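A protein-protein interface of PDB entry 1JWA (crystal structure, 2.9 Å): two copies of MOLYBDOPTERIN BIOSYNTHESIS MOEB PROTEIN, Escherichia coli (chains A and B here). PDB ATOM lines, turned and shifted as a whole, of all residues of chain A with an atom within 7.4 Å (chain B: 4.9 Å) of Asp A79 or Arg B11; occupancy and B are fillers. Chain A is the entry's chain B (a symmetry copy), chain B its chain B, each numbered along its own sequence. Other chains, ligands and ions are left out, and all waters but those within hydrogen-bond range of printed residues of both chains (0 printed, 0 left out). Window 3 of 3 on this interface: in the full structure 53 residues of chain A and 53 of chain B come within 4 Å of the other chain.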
ATOM      1  N   VAL A  66     -21.026  -6.811  16.405  1.00  0.00           N
ATOM      2  CA  VAL A  66     -21.015  -7.475  15.084  1.00  0.00           C
ATOM      3  C   VAL A  66     -20.243  -8.775  15.150  1.00  0.00           C
ATOM      4  O   VAL A  66     -19.287  -8.904  15.938  1.00  0.00           O
ATOM      5  CB  VAL A  66     -20.294  -6.647  14.022  1.00  0.00           C
ATOM      6  CG1 VAL A  66     -20.556  -7.205  12.661  1.00  0.00           C
ATOM      7  CG2 VAL A  66     -20.665  -5.195  14.133  1.00  0.00           C
ATOM      8  N   SER A  67     -20.637  -9.717  14.304  1.00  0.00           N
ATOM      9  CA  SER A  67     -19.982 -11.006  14.267  1.00  0.00           C
ATOM     10  C   SER A  67     -20.004 -11.607  12.858  1.00  0.00           C
ATOM     11  O   SER A  67     -20.740 -11.163  11.981  1.00  0.00           O
ATOM     12  CB  SER A  67     -20.615 -11.943  15.292  1.00  0.00           C
ATOM     13  OG  SER A  67     -21.789 -12.528  14.790  1.00  0.00           O
ATOM     14  N   LEU A  68     -19.181 -12.620  12.644  1.00  0.00           N
ATOM     15  CA  LEU A  68     -19.075 -13.261  11.340  1.00  0.00           C
ATOM     16  C   LEU A  68     -20.426 -13.689  10.807  1.00  0.00           C
ATOM     17  O   LEU A  68     -20.888 -13.112   9.860  1.00  0.00           O
ATOM     18  CB  LEU A  68     -18.129 -14.445  11.448  1.00  0.00           C
ATOM     19  CG  LEU A  68     -17.576 -15.031  10.174  1.00  0.00           C
ATOM     20  CD1 LEU A  68     -17.243 -13.952   9.160  1.00  0.00           C
ATOM     21  CD2 LEU A  68     -16.365 -15.838  10.515  1.00  0.00           C
ATOM     22  N   SER A  69     -21.048 -14.663  11.461  1.00  0.00           N
ATOM     23  CA  SER A  69     -22.344 -15.163  11.093  1.00  0.00           C
ATOM     24  C   SER A  69     -23.289 -14.065  10.596  1.00  0.00           C
ATOM     25  O   SER A  69     -23.986 -14.261   9.640  1.00  0.00           O
ATOM     26  CB  SER A  69     -22.973 -15.907  12.267  1.00  0.00           C
ATOM     27  OG  SER A  69     -24.319 -15.479  12.443  1.00  0.00           O
ATOM     28  N   ASN A  70     -23.306 -12.913  11.237  1.00  0.00           N
ATOM     29  CA  ASN A  70     -24.163 -11.800  10.854  1.00  0.00           C
ATOM     30  C   ASN A  70     -23.947 -11.258   9.456  1.00  0.00           C
ATOM     31  O   ASN A  70     -24.832 -10.609   8.906  1.00  0.00           O
ATOM     32  CB  ASN A  70     -23.933 -10.636  11.808  1.00  0.00           C
ATOM     33  CG  ASN A  70     -24.202 -10.981  13.217  1.00  0.00           C
ATOM     34  OD1 ASN A  70     -23.717 -10.314  14.139  1.00  0.00           O
ATOM     35  ND2 ASN A  70     -24.992 -12.027  13.421  1.00  0.00           N
ATOM     36  N   LEU A  71     -22.756 -11.517   8.913  1.00  0.00           N
ATOM     37  CA  LEU A  71     -22.340 -11.038   7.608  1.00  0.00           C
ATOM     38  C   LEU A  71     -22.930 -11.820   6.449  1.00  0.00           C
ATOM     39  O   LEU A  71     -22.552 -11.626   5.289  1.00  0.00           O
ATOM     40  CB  LEU A  71     -20.820 -11.052   7.515  1.00  0.00           C
ATOM     41  CG  LEU A  71     -20.023 -10.395   8.640  1.00  0.00           C
ATOM     42  CD1 LEU A  71     -18.571 -10.360   8.230  1.00  0.00           C
ATOM     43  CD2 LEU A  71     -20.522  -9.022   8.954  1.00  0.00           C
ATOM     44  N   GLN A  72     -23.867 -12.704   6.740  1.00  0.00           N
ATOM     45  CA  GLN A  72     -24.569 -13.461   5.693  1.00  0.00           C
ATOM     46  C   GLN A  72     -25.800 -12.694   5.304  1.00  0.00           C
ATOM     47  O   GLN A  72     -26.413 -12.956   4.297  1.00  0.00           O
ATOM     48  CB  GLN A  72     -24.930 -14.866   6.211  1.00  0.00           C
ATOM     49  CG  GLN A  72     -26.194 -15.528   5.591  1.00  0.00           C
ATOM     50  CD  GLN A  72     -27.411 -15.479   6.516  1.00  0.00           C
ATOM     51  OE1 GLN A  72     -27.297 -15.104   7.662  1.00  0.00           O
ATOM     52  NE2 GLN A  72     -28.549 -15.876   6.028  1.00  0.00           N
ATOM     53  N   ARG A  73     -26.149 -11.694   6.091  1.00  0.00           N
ATOM     54  CA  ARG A  73     -27.362 -10.957   5.818  1.00  0.00           C
ATOM     55  C   ARG A  73     -27.348  -9.499   6.232  1.00  0.00           C
ATOM     56  O   ARG A  73     -28.070  -8.714   5.660  1.00  0.00           O
ATOM     57  CB  ARG A  73     -28.555 -11.696   6.441  1.00  0.00           C
ATOM     58  CG  ARG A  73     -28.702 -11.588   7.955  1.00  0.00           C
ATOM     59  CD  ARG A  73     -29.439 -12.758   8.532  1.00  0.00           C
ATOM     60  NE  ARG A  73     -29.624 -12.668   9.962  1.00  0.00           N
ATOM     61  CZ  ARG A  73     -28.740 -13.056  10.873  1.00  0.00           C
ATOM     62  NH1 ARG A  73     -27.581 -13.584  10.520  1.00  0.00           N
ATOM     63  NH2 ARG A  73     -29.003 -12.886  12.157  1.00  0.00           N
ATOM     64  N   HIS A  77     -22.936  -4.022   8.028  1.00  0.00           N
ATOM     65  CA  HIS A  77     -21.723  -4.397   8.776  1.00  0.00           C
ATOM     66  C   HIS A  77     -20.717  -5.031   7.863  1.00  0.00           C
ATOM     67  O   HIS A  77     -21.060  -5.333   6.728  1.00  0.00           O
ATOM     68  CB  HIS A  77     -22.038  -5.374   9.901  1.00  0.00           C
ATOM     69  CG  HIS A  77     -23.123  -4.917  10.821  1.00  0.00           C
ATOM     70  ND1 HIS A  77     -23.175  -3.639  11.334  1.00  0.00           N
ATOM     71  CD2 HIS A  77     -24.101  -5.612  11.452  1.00  0.00           C
ATOM     72  CE1 HIS A  77     -24.247  -3.530  12.100  1.00  0.00           C
ATOM     73  NE2 HIS A  77     -24.821  -4.708  12.203  1.00  0.00           N
ATOM     74  N   SER A  78     -19.476  -5.199   8.344  1.00  0.00           N
ATOM     75  CA  SER A  78     -18.419  -5.805   7.539  1.00  0.00           C
ATOM     76  C   SER A  78     -17.371  -6.494   8.365  1.00  0.00           C
ATOM     77  O   SER A  78     -17.295  -6.320   9.553  1.00  0.00           O
ATOM     78  CB  SER A  78     -17.738  -4.757   6.715  1.00  0.00           C
ATOM     79  OG  SER A  78     -17.175  -3.823   7.568  1.00  0.00           O
ATOM     80  N   ASP A  79     -16.539  -7.283   7.713  1.00  0.00           N
ATOM     81  CA  ASP A  79     -15.483  -8.018   8.391  1.00  0.00           C
ATOM     82  C   ASP A  79     -14.635  -7.030   9.195  1.00  0.00           C
ATOM     83  O   ASP A  79     -14.261  -7.263  10.291  1.00  0.00           O
ATOM     84  CB  ASP A  79     -14.585  -8.747   7.358  1.00  0.00           C
ATOM     85  CG  ASP A  79     -15.349  -9.700   6.507  1.00  0.00           C
ATOM     86  OD1 ASP A  79     -15.608  -9.342   5.342  1.00  0.00           O
ATOM     87  OD2 ASP A  79     -15.755 -10.819   6.909  1.00  0.00           O
ATOM     88  N   ALA A  80     -14.312  -5.908   8.619  1.00  0.00           N
ATOM     89  CA  ALA A  80     -13.506  -4.954   9.329  1.00  0.00           C
ATOM     90  C   ALA A  80     -14.151  -4.438  10.608  1.00  0.00           C
ATOM     91  O   ALA A  80     -13.431  -3.952  11.492  1.00  0.00           O
ATOM     92  CB  ALA A  80     -13.226  -3.815   8.428  1.00  0.00           C
ATOM     93  N   THR A  81     -15.484  -4.507  10.718  1.00  0.00           N
ATOM     94  CA  THR A  81     -16.197  -4.061  11.936  1.00  0.00           C
ATOM     95  C   THR A  81     -16.613  -5.187  12.934  1.00  0.00           C
ATOM     96  O   THR A  81     -17.261  -4.939  13.968  1.00  0.00           O
ATOM     97  CB  THR A  81     -17.423  -3.169  11.601  1.00  0.00           C
ATOM     98  OG1 THR A  81     -18.555  -3.938  11.148  1.00  0.00           O
ATOM     99  CG2 THR A  81     -17.089  -2.312  10.519  1.00  0.00           C
ATOM    100  N   VAL A  82     -16.238  -6.417  12.632  1.00  0.00           N
ATOM    101  CA  VAL A  82     -16.574  -7.519  13.522  1.00  0.00           C
ATOM    102  C   VAL A  82     -16.038  -7.194  14.912  1.00  0.00           C
ATOM    103  O   VAL A  82     -14.903  -6.790  15.072  1.00  0.00           O
ATOM    104  CB  VAL A  82     -15.988  -8.853  13.014  1.00  0.00           C
ATOM    105  CG1 VAL A  82     -16.393  -9.985  13.900  1.00  0.00           C
ATOM    106  CG2 VAL A  82     -16.455  -9.122  11.578  1.00  0.00           C
ATOM    107  N   GLY A  83     -16.868  -7.336  15.922  1.00  0.00           N
ATOM    108  CA  GLY A  83     -16.433  -7.032  17.255  1.00  0.00           C
ATOM    109  C   GLY A  83     -16.915  -5.703  17.723  1.00  0.00           C
ATOM    110  O   GLY A  83     -17.338  -5.532  18.837  1.00  0.00           O
ATOM    111  N   GLN B   7     -14.143 -21.001   7.372  1.00  0.00           N
ATOM    112  CA  GLN B   7     -14.625 -19.623   7.521  1.00  0.00           C
ATOM    113  C   GLN B   7     -15.921 -19.423   6.759  1.00  0.00           C
ATOM    114  O   GLN B   7     -16.837 -18.745   7.221  1.00  0.00           O
ATOM    115  CB  GLN B   7     -13.565 -18.637   7.060  1.00  0.00           C
ATOM    116  CG  GLN B   7     -12.495 -19.259   6.196  1.00  0.00           C
ATOM    117  CD  GLN B   7     -11.413 -19.866   7.025  1.00  0.00           C
ATOM    118  OE1 GLN B   7     -10.815 -20.866   6.636  1.00  0.00           O
ATOM    119  NE2 GLN B   7     -11.147 -19.254   8.185  1.00  0.00           N
ATOM    120  N   GLU B   8     -16.021 -20.019   5.589  1.00  0.00           N
ATOM    121  CA  GLU B   8     -17.264 -19.893   4.850  1.00  0.00           C
ATOM    122  C   GLU B   8     -18.327 -20.599   5.700  1.00  0.00           C
ATOM    123  O   GLU B   8     -19.400 -20.081   5.964  1.00  0.00           O
ATOM    124  CB  GLU B   8     -17.143 -20.530   3.452  1.00  0.00           C
ATOM    125  CG  GLU B   8     -16.017 -19.917   2.621  1.00  0.00           C
ATOM    126  CD  GLU B   8     -16.006 -20.331   1.158  1.00  0.00           C
ATOM    127  OE1 GLU B   8     -15.777 -21.509   0.887  1.00  0.00           O
ATOM    128  OE2 GLU B   8     -16.224 -19.479   0.282  1.00  0.00           O
ATOM    129  N   MET B   9     -17.987 -21.793   6.146  1.00  0.00           N
ATOM    130  CA  MET B   9     -18.916 -22.603   6.915  1.00  0.00           C
ATOM    131  C   MET B   9     -19.400 -21.892   8.154  1.00  0.00           C
ATOM    132  O   MET B   9     -20.471 -22.212   8.636  1.00  0.00           O
ATOM    133  CB  MET B   9     -18.294 -23.957   7.280  1.00  0.00           C
ATOM    134  CG  MET B   9     -18.150 -24.901   6.089  1.00  0.00           C
ATOM    135  SD  MET B   9     -17.855 -26.633   6.529  1.00  0.00           S
ATOM    136  CE  MET B   9     -16.201 -26.556   7.090  1.00  0.00           C
ATOM    137  N   LEU B  10     -18.664 -20.911   8.657  1.00  0.00           N
ATOM    138  CA  LEU B  10     -19.148 -20.199   9.836  1.00  0.00           C
ATOM    139  C   LEU B  10     -20.016 -19.007   9.442  1.00  0.00           C
ATOM    140  O   LEU B  10     -21.096 -18.800   9.985  1.00  0.00           O
ATOM    141  CB  LEU B  10     -18.000 -19.705  10.686  1.00  0.00           C
ATOM    142  CG  LEU B  10     -17.074 -20.756  11.367  1.00  0.00           C
ATOM    143  CD1 LEU B  10     -16.383 -20.166  12.619  1.00  0.00           C
ATOM    144  CD2 LEU B  10     -17.803 -22.076  11.736  1.00  0.00           C
ATOM    145  N   ARG B  11     -19.562 -18.249   8.443  1.00  0.00           N
ATOM    146  CA  ARG B  11     -20.284 -17.130   7.949  1.00  0.00           C
ATOM    147  C   ARG B  11     -21.628 -17.535   7.351  1.00  0.00           C
ATOM    148  O   ARG B  11     -22.617 -16.802   7.468  1.00  0.00           O
ATOM    149  CB  ARG B  11     -19.415 -16.459   6.887  1.00  0.00           C
ATOM    150  CG  ARG B  11     -20.050 -15.315   6.077  1.00  0.00           C
ATOM    151  CD  ARG B  11     -19.205 -14.962   4.896  1.00  0.00           C
ATOM    152  NE  ARG B  11     -19.101 -13.528   4.627  1.00  0.00           N
ATOM    153  CZ  ARG B  11     -18.080 -12.751   4.957  1.00  0.00           C
ATOM    154  NH1 ARG B  11     -17.034 -13.245   5.550  1.00  0.00           N
ATOM    155  NH2 ARG B  11     -18.101 -11.462   4.678  1.00  0.00           N
ATOM    156  N   TYR B  12     -21.686 -18.666   6.683  1.00  0.00           N
ATOM    157  CA  TYR B  12     -22.923 -19.068   6.037  1.00  0.00           C
ATOM    158  C   TYR B  12     -23.863 -19.922   6.903  1.00  0.00           C
ATOM    159  O   TYR B  12     -24.960 -20.339   6.458  1.00  0.00           O
ATOM    160  CB  TYR B  12     -22.600 -19.822   4.770  1.00  0.00           C
ATOM    161  CG  TYR B  12     -21.888 -18.987   3.710  1.00  0.00           C
ATOM    162  CD1 TYR B  12     -20.878 -19.517   2.922  1.00  0.00           C
ATOM    163  CD2 TYR B  12     -22.207 -17.689   3.505  1.00  0.00           C
ATOM    164  CE1 TYR B  12     -20.233 -18.753   1.984  1.00  0.00           C
ATOM    165  CE2 TYR B  12     -21.570 -16.957   2.554  1.00  0.00           C
ATOM    166  CZ  TYR B  12     -20.596 -17.479   1.815  1.00  0.00           C
ATOM    167  OH  TYR B  12     -20.016 -16.665   0.880  1.00  0.00           O
ATOM    168  N   ASN B  13     -23.438 -20.163   8.143  1.00  0.00           N
ATOM    169  CA  ASN B  13     -24.164 -20.995   9.100  1.00  0.00           C
ATOM    170  C   ASN B  13     -25.670 -20.915   9.121  1.00  0.00           C
ATOM    171  O   ASN B  13     -26.340 -21.919   8.907  1.00  0.00           O
ATOM    172  CB  ASN B  13     -23.634 -20.711  10.522  1.00  0.00           C
ATOM    173  CG  ASN B  13     -24.347 -21.524  11.575  1.00  0.00           C
ATOM    174  OD1 ASN B  13     -25.396 -21.143  12.053  1.00  0.00           O
ATOM    175  ND2 ASN B  13     -23.803 -22.662  11.898  1.00  0.00           N
ATOM    176  N   ARG B  96     -16.937  -5.661  -0.617  1.00  0.00           N
ATOM    177  CA  ARG B  96     -16.793  -5.279   0.769  1.00  0.00           C
ATOM    178  C   ARG B  96     -17.742  -6.154   1.544  1.00  0.00           C
ATOM    179  O   ARG B  96     -17.421  -6.557   2.629  1.00  0.00           O
ATOM    180  CB  ARG B  96     -17.206  -3.846   0.969  1.00  0.00           C
ATOM    181  CG  ARG B  96     -16.238  -3.013   1.730  1.00  0.00           C
ATOM    182  CD  ARG B  96     -15.626  -1.865   0.872  1.00  0.00           C
ATOM    183  NE  ARG B  96     -16.067  -0.550   1.330  1.00  0.00           N
ATOM    184  CZ  ARG B  96     -17.351  -0.136   1.356  1.00  0.00           C
ATOM    185  NH1 ARG B  96     -18.381  -0.895   0.949  1.00  0.00           N
ATOM    186  NH2 ARG B  96     -17.598   1.082   1.801  1.00  0.00           N
ATOM    187  N   ILE B  97     -18.929  -6.386   1.000  1.00  0.00           N
ATOM    188  CA  ILE B  97     -19.928  -7.196   1.642  1.00  0.00           C
ATOM    189  C   ILE B  97     -19.464  -8.615   1.697  1.00  0.00           C
ATOM    190  O   ILE B  97     -19.682  -9.257   2.692  1.00  0.00           O
ATOM    191  CB  ILE B  97     -21.268  -7.152   0.878  1.00  0.00           C
ATOM    192  CG1 ILE B  97     -21.911  -5.789   0.997  1.00  0.00           C
ATOM    193  CG2 ILE B  97     -22.211  -8.223   1.398  1.00  0.00           C
ATOM    194  CD1 ILE B  97     -23.232  -5.599   0.197  1.00  0.00           C
ATOM    195  N   ASN B  98     -18.831  -9.110   0.635  1.00  0.00           N
ATOM    196  CA  ASN B  98     -18.291 -10.482   0.644  1.00  0.00           C
ATOM    197  C   ASN B  98     -17.023 -10.666  -0.196  1.00  0.00           C
ATOM    198  O   ASN B  98     -17.088 -10.743  -1.425  1.00  0.00           O
ATOM    199  CB  ASN B  98     -19.333 -11.459   0.145  1.00  0.00           C
ATOM    200  CG  ASN B  98     -19.058 -12.853   0.581  1.00  0.00           C
ATOM    201  OD1 ASN B  98     -17.972 -13.138   1.059  1.00  0.00           O
ATOM    202  ND2 ASN B  98     -20.050 -13.739   0.445  1.00  0.00           N
ATOM    203  N   PRO B  99     -15.871 -10.720   0.478  1.00  0.00           N
ATOM    204  CA  PRO B  99     -14.590 -10.895  -0.192  1.00  0.00           C
ATOM    205  C   PRO B  99     -14.375 -12.323  -0.632  1.00  0.00           C
ATOM    206  O   PRO B  99     -13.377 -12.624  -1.266  1.00  0.00           O
ATOM    207  CB  PRO B  99     -13.590 -10.480   0.842  1.00  0.00           C
ATOM    208  CG  PRO B  99     -14.217 -10.737   2.096  1.00  0.00           C
ATOM    209  CD  PRO B  99     -15.691 -10.561   1.923  1.00  0.00           C
ATOM    210  N   HIS B 100     -15.349 -13.173  -0.412  1.00  0.00           N
ATOM    211  CA  HIS B 100     -15.226 -14.553  -0.826  1.00  0.00           C
ATOM    212  C   HIS B 100     -15.672 -14.893  -2.266  1.00  0.00           C
ATOM    213  O   HIS B 100     -15.221 -15.924  -2.830  1.00  0.00           O
ATOM    214  CB  HIS B 100     -16.006 -15.417   0.157  1.00  0.00           C
ATOM    215  CG  HIS B 100     -15.350 -15.538   1.493  1.00  0.00           C
ATOM    216  ND1 HIS B 100     -14.091 -16.077   1.638  1.00  0.00           N
ATOM    217  CD2 HIS B 100     -15.820 -15.317   2.754  1.00  0.00           C
ATOM    218  CE1 HIS B 100     -13.820 -16.166   2.936  1.00  0.00           C
ATOM    219  NE2 HIS B 100     -14.916 -15.876   3.623  1.00  0.00           N
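Arg B11 touches just these residues of chain A: Leu A68, Ser A69, Leu A71, Gln A72 and Asp A79.
Of the printed residues of chain B, Leu A68 touches Arg B11.
Of the printed residues of chain B, Leu A71 touches Arg B11 (3.7 Å).
The nearest residue of chain A that does not touch Arg B11 is Asn A70 (5.5 Å).
The guanidinium group (NH1) of Arg B11 is in salt-bridge range of the side-chain carboxylate (OD2) of Asp A79, at 3.1 Å.
No position is printed for both chains.
The backbone carbonyl oxygen (O) of Ile B97 lies within hydrogen-bond range of the guanidinium group (NH2) of Arg B11, 3.4 Å away.
OE1 of Gln A72 sits at hydrogen-bond distance from NH1 of Arg A73 (3.2 Å).
Arg B11 touches Leu A68 (NH1 to CD1, 3.7 Å).
Ser A69 touches Arg B11 (O to O, 3.6 Å).
Leu A71 touches Arg B11.
CB of Gln A72 touches O of Arg B11 (3.3 Å).
Asp A79 touches Pro B99.
Hydrophobic or aromatic side chains of chain A that line the printed part of chain B: Leu A68 and Leu A71.
Of the 12 printed residues of chain B, 2 touch a printed residue of chain A.
Hydrophobic or aromatic side chains of chain B that line the printed part of chain A: Pro B99.
Among the printed residues, 6 pairs touch across the chains.
Among the printed residues, Asp or Glu carboxylates within 4 Å of a Lys or Arg side-chain nitrogen of the other chain: Asp A79 with Arg B11 (3.1 Å).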
